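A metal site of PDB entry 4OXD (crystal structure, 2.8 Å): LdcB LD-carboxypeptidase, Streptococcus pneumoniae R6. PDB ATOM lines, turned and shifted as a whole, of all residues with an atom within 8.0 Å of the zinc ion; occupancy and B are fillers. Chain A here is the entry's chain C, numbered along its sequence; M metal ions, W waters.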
ATOM      1  N   SER A  66     -18.805 -19.814  29.661  1.00  0.00           N
ATOM      2  CA  SER A  66     -19.776 -20.699  28.990  1.00  0.00           C
ATOM      3  C   SER A  66     -19.406 -20.855  27.514  1.00  0.00           C
ATOM      4  O   SER A  66     -19.883 -20.105  26.659  1.00  0.00           O
ATOM      5  CB  SER A  66     -21.202 -20.163  29.125  1.00  0.00           C
ATOM      6  OG  SER A  66     -21.551 -19.973  30.484  1.00  0.00           O
ATOM      7  N   GLY A  67     -18.557 -21.834  27.225  1.00  0.00           N
ATOM      8  CA  GLY A  67     -18.037 -22.030  25.879  1.00  0.00           C
ATOM      9  C   GLY A  67     -18.979 -22.815  24.975  1.00  0.00           C
ATOM     10  O   GLY A  67     -20.112 -22.406  24.731  1.00  0.00           O
ATOM     11  N   ARG A  69     -21.543 -25.507  23.553  1.00  0.00           N
ATOM     12  CA  ARG A  69     -22.716 -26.272  23.992  1.00  0.00           C
ATOM     13  C   ARG A  69     -23.357 -26.992  22.800  1.00  0.00           C
ATOM     14  O   ARG A  69     -23.817 -26.356  21.851  1.00  0.00           O
ATOM     15  CB  ARG A  69     -23.741 -25.363  24.683  1.00  0.00           C
ATOM     16  CG  ARG A  69     -23.338 -24.932  26.078  1.00  0.00           C
ATOM     17  CD  ARG A  69     -24.497 -24.346  26.880  1.00  0.00           C
ATOM     18  NE  ARG A  69     -24.905 -23.023  26.403  1.00  0.00           N
ATOM     19  CZ  ARG A  69     -25.770 -22.213  27.027  1.00  0.00           C
ATOM     20  NH1 ARG A  69     -26.064 -21.028  26.505  1.00  0.00           N
ATOM     21  NH2 ARG A  69     -26.340 -22.587  28.173  1.00  0.00           N
ATOM     22  N   SER A 100     -28.739 -22.082  18.362  1.00  0.00           N
ATOM     23  CA  SER A 100     -27.861 -21.381  19.301  1.00  0.00           C
ATOM     24  C   SER A 100     -26.479 -21.166  18.716  1.00  0.00           C
ATOM     25  O   SER A 100     -25.942 -22.030  18.021  1.00  0.00           O
ATOM     26  CB  SER A 100     -27.734 -22.169  20.604  1.00  0.00           C
ATOM     27  OG  SER A 100     -26.919 -21.480  21.531  1.00  0.00           O
ATOM     28  N   GLU A 101     -25.893 -20.017  19.030  1.00  0.00           N
ATOM     29  CA  GLU A 101     -24.548 -19.680  18.572  1.00  0.00           C
ATOM     30  C   GLU A 101     -23.470 -20.448  19.325  1.00  0.00           C
ATOM     31  O   GLU A 101     -22.349 -20.600  18.835  1.00  0.00           O
ATOM     32  CB  GLU A 101     -24.316 -18.172  18.729  1.00  0.00           C
ATOM     33  CG  GLU A 101     -23.296 -17.602  17.775  1.00  0.00           C
ATOM     34  CD  GLU A 101     -23.248 -16.087  17.827  1.00  0.00           C
ATOM     35  OE1 GLU A 101     -23.292 -15.528  18.939  1.00  0.00           O
ATOM     36  OE2 GLU A 101     -23.158 -15.456  16.745  1.00  0.00           O
ATOM     37  N   HIS A 102     -23.803 -20.929  20.531  1.00  0.00           N
ATOM     38  CA  HIS A 102     -22.876 -21.711  21.340  1.00  0.00           C
ATOM     39  C   HIS A 102     -22.537 -23.074  20.752  1.00  0.00           C
ATOM     40  O   HIS A 102     -21.542 -23.679  21.139  1.00  0.00           O
ATOM     41  CB  HIS A 102     -23.446 -21.913  22.741  1.00  0.00           C
ATOM     42  CG  HIS A 102     -23.431 -20.685  23.592  1.00  0.00           C
ATOM     43  ND1 HIS A 102     -22.445 -20.433  24.517  1.00  0.00           N
ATOM     44  CD2 HIS A 102     -24.277 -19.639  23.642  1.00  0.00           C
ATOM     45  CE1 HIS A 102     -22.706 -19.289  25.132  1.00  0.00           C
ATOM     46  NE2 HIS A 102     -23.772 -18.752  24.562  1.00  0.00           N
ATOM     47  N   ALA A 107     -18.858 -18.850  20.086  1.00  0.00           N
ATOM     48  CA  ALA A 107     -19.588 -18.037  21.054  1.00  0.00           C
ATOM     49  C   ALA A 107     -19.214 -18.437  22.477  1.00  0.00           C
ATOM     50  O   ALA A 107     -19.282 -19.616  22.832  1.00  0.00           O
ATOM     51  CB  ALA A 107     -21.086 -18.171  20.847  1.00  0.00           C
ATOM     52  N   PHE A 108     -18.817 -17.450  23.281  1.00  0.00           N
ATOM     53  CA  PHE A 108     -18.452 -17.672  24.682  1.00  0.00           C
ATOM     54  C   PHE A 108     -19.124 -16.597  25.535  1.00  0.00           C
ATOM     55  O   PHE A 108     -19.183 -15.436  25.126  1.00  0.00           O
ATOM     56  CB  PHE A 108     -16.931 -17.570  24.856  1.00  0.00           C
ATOM     57  CG  PHE A 108     -16.151 -18.472  23.945  1.00  0.00           C
ATOM     58  CD1 PHE A 108     -15.884 -18.104  22.631  1.00  0.00           C
ATOM     59  CD2 PHE A 108     -15.660 -19.685  24.394  1.00  0.00           C
ATOM     60  CE1 PHE A 108     -15.160 -18.934  21.790  1.00  0.00           C
ATOM     61  CE2 PHE A 108     -14.938 -20.522  23.568  1.00  0.00           C
ATOM     62  CZ  PHE A 108     -14.682 -20.147  22.257  1.00  0.00           C
ATOM     63  N   ASP A 109     -19.636 -16.992  26.695  1.00  0.00           N
ATOM     64  CA  ASP A 109     -20.173 -16.033  27.671  1.00  0.00           C
ATOM     65  C   ASP A 109     -19.170 -15.822  28.784  1.00  0.00           C
ATOM     66  O   ASP A 109     -18.660 -16.779  29.369  1.00  0.00           O
ATOM     67  CB  ASP A 109     -21.498 -16.501  28.290  1.00  0.00           C
ATOM     68  CG  ASP A 109     -22.587 -16.796  27.263  1.00  0.00           C
ATOM     69  OD1 ASP A 109     -22.533 -16.246  26.144  1.00  0.00           O
ATOM     70  OD2 ASP A 109     -23.502 -17.574  27.590  1.00  0.00           O
ATOM     71  N   VAL A 110     -18.883 -14.556  29.077  1.00  0.00           N
ATOM     72  CA  VAL A 110     -18.079 -14.192  30.236  1.00  0.00           C
ATOM     73  C   VAL A 110     -18.954 -14.347  31.490  1.00  0.00           C
ATOM     74  O   VAL A 110     -20.164 -14.112  31.443  1.00  0.00           O
ATOM     75  CB  VAL A 110     -17.556 -12.750  30.127  1.00  0.00           C
ATOM     76  CG1 VAL A 110     -16.879 -12.307  31.405  1.00  0.00           C
ATOM     77  CG2 VAL A 110     -16.584 -12.623  28.960  1.00  0.00           C
ATOM     78  N   ARG A 139     -22.510  -9.648  20.498  1.00  0.00           N
ATOM     79  CA  ARG A 139     -23.435 -10.125  19.472  1.00  0.00           C
ATOM     80  C   ARG A 139     -24.809  -9.488  19.618  1.00  0.00           C
ATOM     81  O   ARG A 139     -25.323  -8.879  18.670  1.00  0.00           O
ATOM     82  CB  ARG A 139     -23.564 -11.656  19.560  1.00  0.00           C
ATOM     83  CG  ARG A 139     -24.326 -12.304  18.419  1.00  0.00           C
ATOM     84  CD  ARG A 139     -23.489 -12.388  17.158  1.00  0.00           C
ATOM     85  NE  ARG A 139     -24.191 -13.071  16.075  1.00  0.00           N
ATOM     86  CZ  ARG A 139     -25.142 -12.526  15.314  1.00  0.00           C
ATOM     87  NH1 ARG A 139     -25.697 -13.250  14.347  1.00  0.00           N
ATOM     88  NH2 ARG A 139     -25.534 -11.274  15.503  1.00  0.00           N
ATOM     89  N   TYR A 140     -25.393  -9.633  20.800  1.00  0.00           N
ATOM     90  CA  TYR A 140     -26.746  -9.152  21.109  1.00  0.00           C
ATOM     91  C   TYR A 140     -26.666  -7.794  21.804  1.00  0.00           C
ATOM     92  O   TYR A 140     -26.655  -7.707  23.036  1.00  0.00           O
ATOM     93  CB  TYR A 140     -27.487 -10.172  21.973  1.00  0.00           C
ATOM     94  CG  TYR A 140     -27.331 -11.596  21.474  1.00  0.00           C
ATOM     95  CD1 TYR A 140     -27.582 -11.926  20.151  1.00  0.00           C
ATOM     96  CD2 TYR A 140     -26.933 -12.615  22.342  1.00  0.00           C
ATOM     97  CE1 TYR A 140     -27.430 -13.222  19.683  1.00  0.00           C
ATOM     98  CE2 TYR A 140     -26.790 -13.916  21.884  1.00  0.00           C
ATOM     99  CZ  TYR A 140     -27.043 -14.221  20.560  1.00  0.00           C
ATOM    100  OH  TYR A 140     -26.899 -15.509  20.109  1.00  0.00           O
ATOM    101  N   TYR A 150     -32.656 -11.823  19.650  1.00  0.00           N
ATOM    102  CA  TYR A 150     -32.475 -12.071  21.072  1.00  0.00           C
ATOM    103  C   TYR A 150     -32.525 -10.751  21.834  1.00  0.00           C
ATOM    104  O   TYR A 150     -32.042  -9.733  21.346  1.00  0.00           O
ATOM    105  CB  TYR A 150     -31.124 -12.741  21.323  1.00  0.00           C
ATOM    106  CG  TYR A 150     -30.956 -14.108  20.678  1.00  0.00           C
ATOM    107  CD1 TYR A 150     -30.747 -14.228  19.302  1.00  0.00           C
ATOM    108  CD2 TYR A 150     -30.974 -15.277  21.444  1.00  0.00           C
ATOM    109  CE1 TYR A 150     -30.581 -15.474  18.718  1.00  0.00           C
ATOM    110  CE2 TYR A 150     -30.819 -16.516  20.863  1.00  0.00           C
ATOM    111  CZ  TYR A 150     -30.620 -16.616  19.496  1.00  0.00           C
ATOM    112  OH  TYR A 150     -30.449 -17.854  18.911  1.00  0.00           O
ATOM    113  N   GLU A 153     -27.887  -8.660  25.618  1.00  0.00           N
ATOM    114  CA  GLU A 153     -27.066  -9.478  26.516  1.00  0.00           C
ATOM    115  C   GLU A 153     -25.662  -8.862  26.594  1.00  0.00           C
ATOM    116  O   GLU A 153     -25.004  -8.659  25.565  1.00  0.00           O
ATOM    117  CB  GLU A 153     -27.009 -10.916  26.001  1.00  0.00           C
ATOM    118  CG  GLU A 153     -26.104 -11.873  26.766  1.00  0.00           C
ATOM    119  CD  GLU A 153     -26.481 -12.025  28.223  1.00  0.00           C
ATOM    120  OE1 GLU A 153     -25.571 -12.321  29.034  1.00  0.00           O
ATOM    121  OE2 GLU A 153     -27.668 -11.865  28.555  1.00  0.00           O
ATOM    122  N   TRP A 155     -22.752  -9.930  28.132  1.00  0.00           N
ATOM    123  CA  TRP A 155     -21.547 -10.758  28.232  1.00  0.00           C
ATOM    124  C   TRP A 155     -21.474 -11.917  27.229  1.00  0.00           C
ATOM    125  O   TRP A 155     -20.589 -12.762  27.342  1.00  0.00           O
ATOM    126  CB  TRP A 155     -21.421 -11.278  29.668  1.00  0.00           C
ATOM    127  CG  TRP A 155     -21.374 -10.177  30.685  1.00  0.00           C
ATOM    128  CD1 TRP A 155     -20.307  -9.341  30.952  1.00  0.00           C
ATOM    129  CD2 TRP A 155     -22.419  -9.762  31.567  1.00  0.00           C
ATOM    130  NE1 TRP A 155     -20.639  -8.455  31.942  1.00  0.00           N
ATOM    131  CE2 TRP A 155     -21.929  -8.684  32.335  1.00  0.00           C
ATOM    132  CE3 TRP A 155     -23.729 -10.206  31.779  1.00  0.00           C
ATOM    133  CZ2 TRP A 155     -22.702  -8.045  33.309  1.00  0.00           C
ATOM    134  CZ3 TRP A 155     -24.503  -9.567  32.753  1.00  0.00           C
ATOM    135  CH2 TRP A 155     -23.988  -8.498  33.500  1.00  0.00           C
ATOM    136  N   HIS A 156     -22.367 -11.940  26.245  1.00  0.00           N
ATOM    137  CA  HIS A 156     -22.293 -12.926  25.168  1.00  0.00           C
ATOM    138  C   HIS A 156     -21.349 -12.385  24.082  1.00  0.00           C
ATOM    139  O   HIS A 156     -21.643 -11.380  23.444  1.00  0.00           O
ATOM    140  CB  HIS A 156     -23.682 -13.206  24.586  1.00  0.00           C
ATOM    141  CG  HIS A 156     -23.678 -14.206  23.469  1.00  0.00           C
ATOM    142  ND1 HIS A 156     -24.304 -15.433  23.566  1.00  0.00           N
ATOM    143  CD2 HIS A 156     -23.112 -14.165  22.246  1.00  0.00           C
ATOM    144  CE1 HIS A 156     -24.135 -16.096  22.432  1.00  0.00           C
ATOM    145  NE2 HIS A 156     -23.405 -15.345  21.613  1.00  0.00           N
ATOM    146  N   LEU A 157     -20.225 -13.071  23.889  1.00  0.00           N
ATOM    147  CA  LEU A 157     -19.232 -12.646  22.898  1.00  0.00           C
ATOM    148  C   LEU A 157     -19.170 -13.600  21.712  1.00  0.00           C
ATOM    149  O   LEU A 157     -19.257 -14.818  21.884  1.00  0.00           O
ATOM    150  CB  LEU A 157     -17.851 -12.561  23.550  1.00  0.00           C
ATOM    151  CG  LEU A 157     -17.718 -11.656  24.782  1.00  0.00           C
ATOM    152  CD1 LEU A 157     -16.306 -11.740  25.339  1.00  0.00           C
ATOM    153  CD2 LEU A 157     -18.077 -10.215  24.440  1.00  0.00           C
ATOM    154  N   ARG A 158     -19.014 -13.047  20.507  1.00  0.00           N
ATOM    155  CA  ARG A 158     -18.917 -13.840  19.282  1.00  0.00           C
ATOM    156  C   ARG A 158     -17.612 -13.515  18.543  1.00  0.00           C
ATOM    157  O   ARG A 158     -17.354 -12.362  18.219  1.00  0.00           O
ATOM    158  CB  ARG A 158     -20.123 -13.576  18.368  1.00  0.00           C
ATOM    159  CG  ARG A 158     -19.962 -14.050  16.927  1.00  0.00           C
ATOM    160  CD  ARG A 158     -19.693 -15.544  16.811  1.00  0.00           C
ATOM    161  NE  ARG A 158     -19.307 -15.924  15.445  1.00  0.00           N
ATOM    162  CZ  ARG A 158     -20.163 -16.175  14.448  1.00  0.00           C
ATOM    163  NH1 ARG A 158     -21.481 -16.098  14.635  1.00  0.00           N
ATOM    164  NH2 ARG A 158     -19.697 -16.508  13.255  1.00  0.00           N
HETATM  165 ZN    ZN M   1     -24.156 -16.795  25.133  1.00  0.00          ZN
HETATM  166  O   HOH W   1     -25.547 -16.201  26.208  1.00  0.00           O
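Water W1 is bound to the zinc ion, at 1.9 Å. The zinc ion is bound by the side-chain carboxylate (OD1) of Asp 109 (2.0 Å). A ring nitrogen (NE2) of His 102 binds the zinc ion (2.1 Å). The zinc ion is bound by ND1 of His 156. The zinc ion has four donor atoms within binding distance. Slightly farther from the zinc ion lies the side-chain carboxylate (OD2) of Asp 109 (2.7 Å).
A ring nitrogen (NE2) of His 156 is in hydrogen-bond range of the side-chain carboxylate (OE1) of Glu 101, at 2.7 Å. N of Ser 66 sits at hydrogen-bond distance from O of Asp 109 (3.1 Å). ND1 of His 102 is in hydrogen-bond range of O of Gly 67 (3.1 Å). The side-chain hydroxyl of Ser 100 lies close to the backbone NH of His 102, 3.3 Å away. The backbone carbonyl oxygen (O) of Ser 66 lies close to a ring nitrogen (ND1) of His 102. The backbone carbonyl oxygen (O) of His 102 is in hydrogen-bond range of the backbone NH (N) of Arg 69 (3.0 Å).
Of the 18 residues printed, 3 come within 4 Å of the zinc ion.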
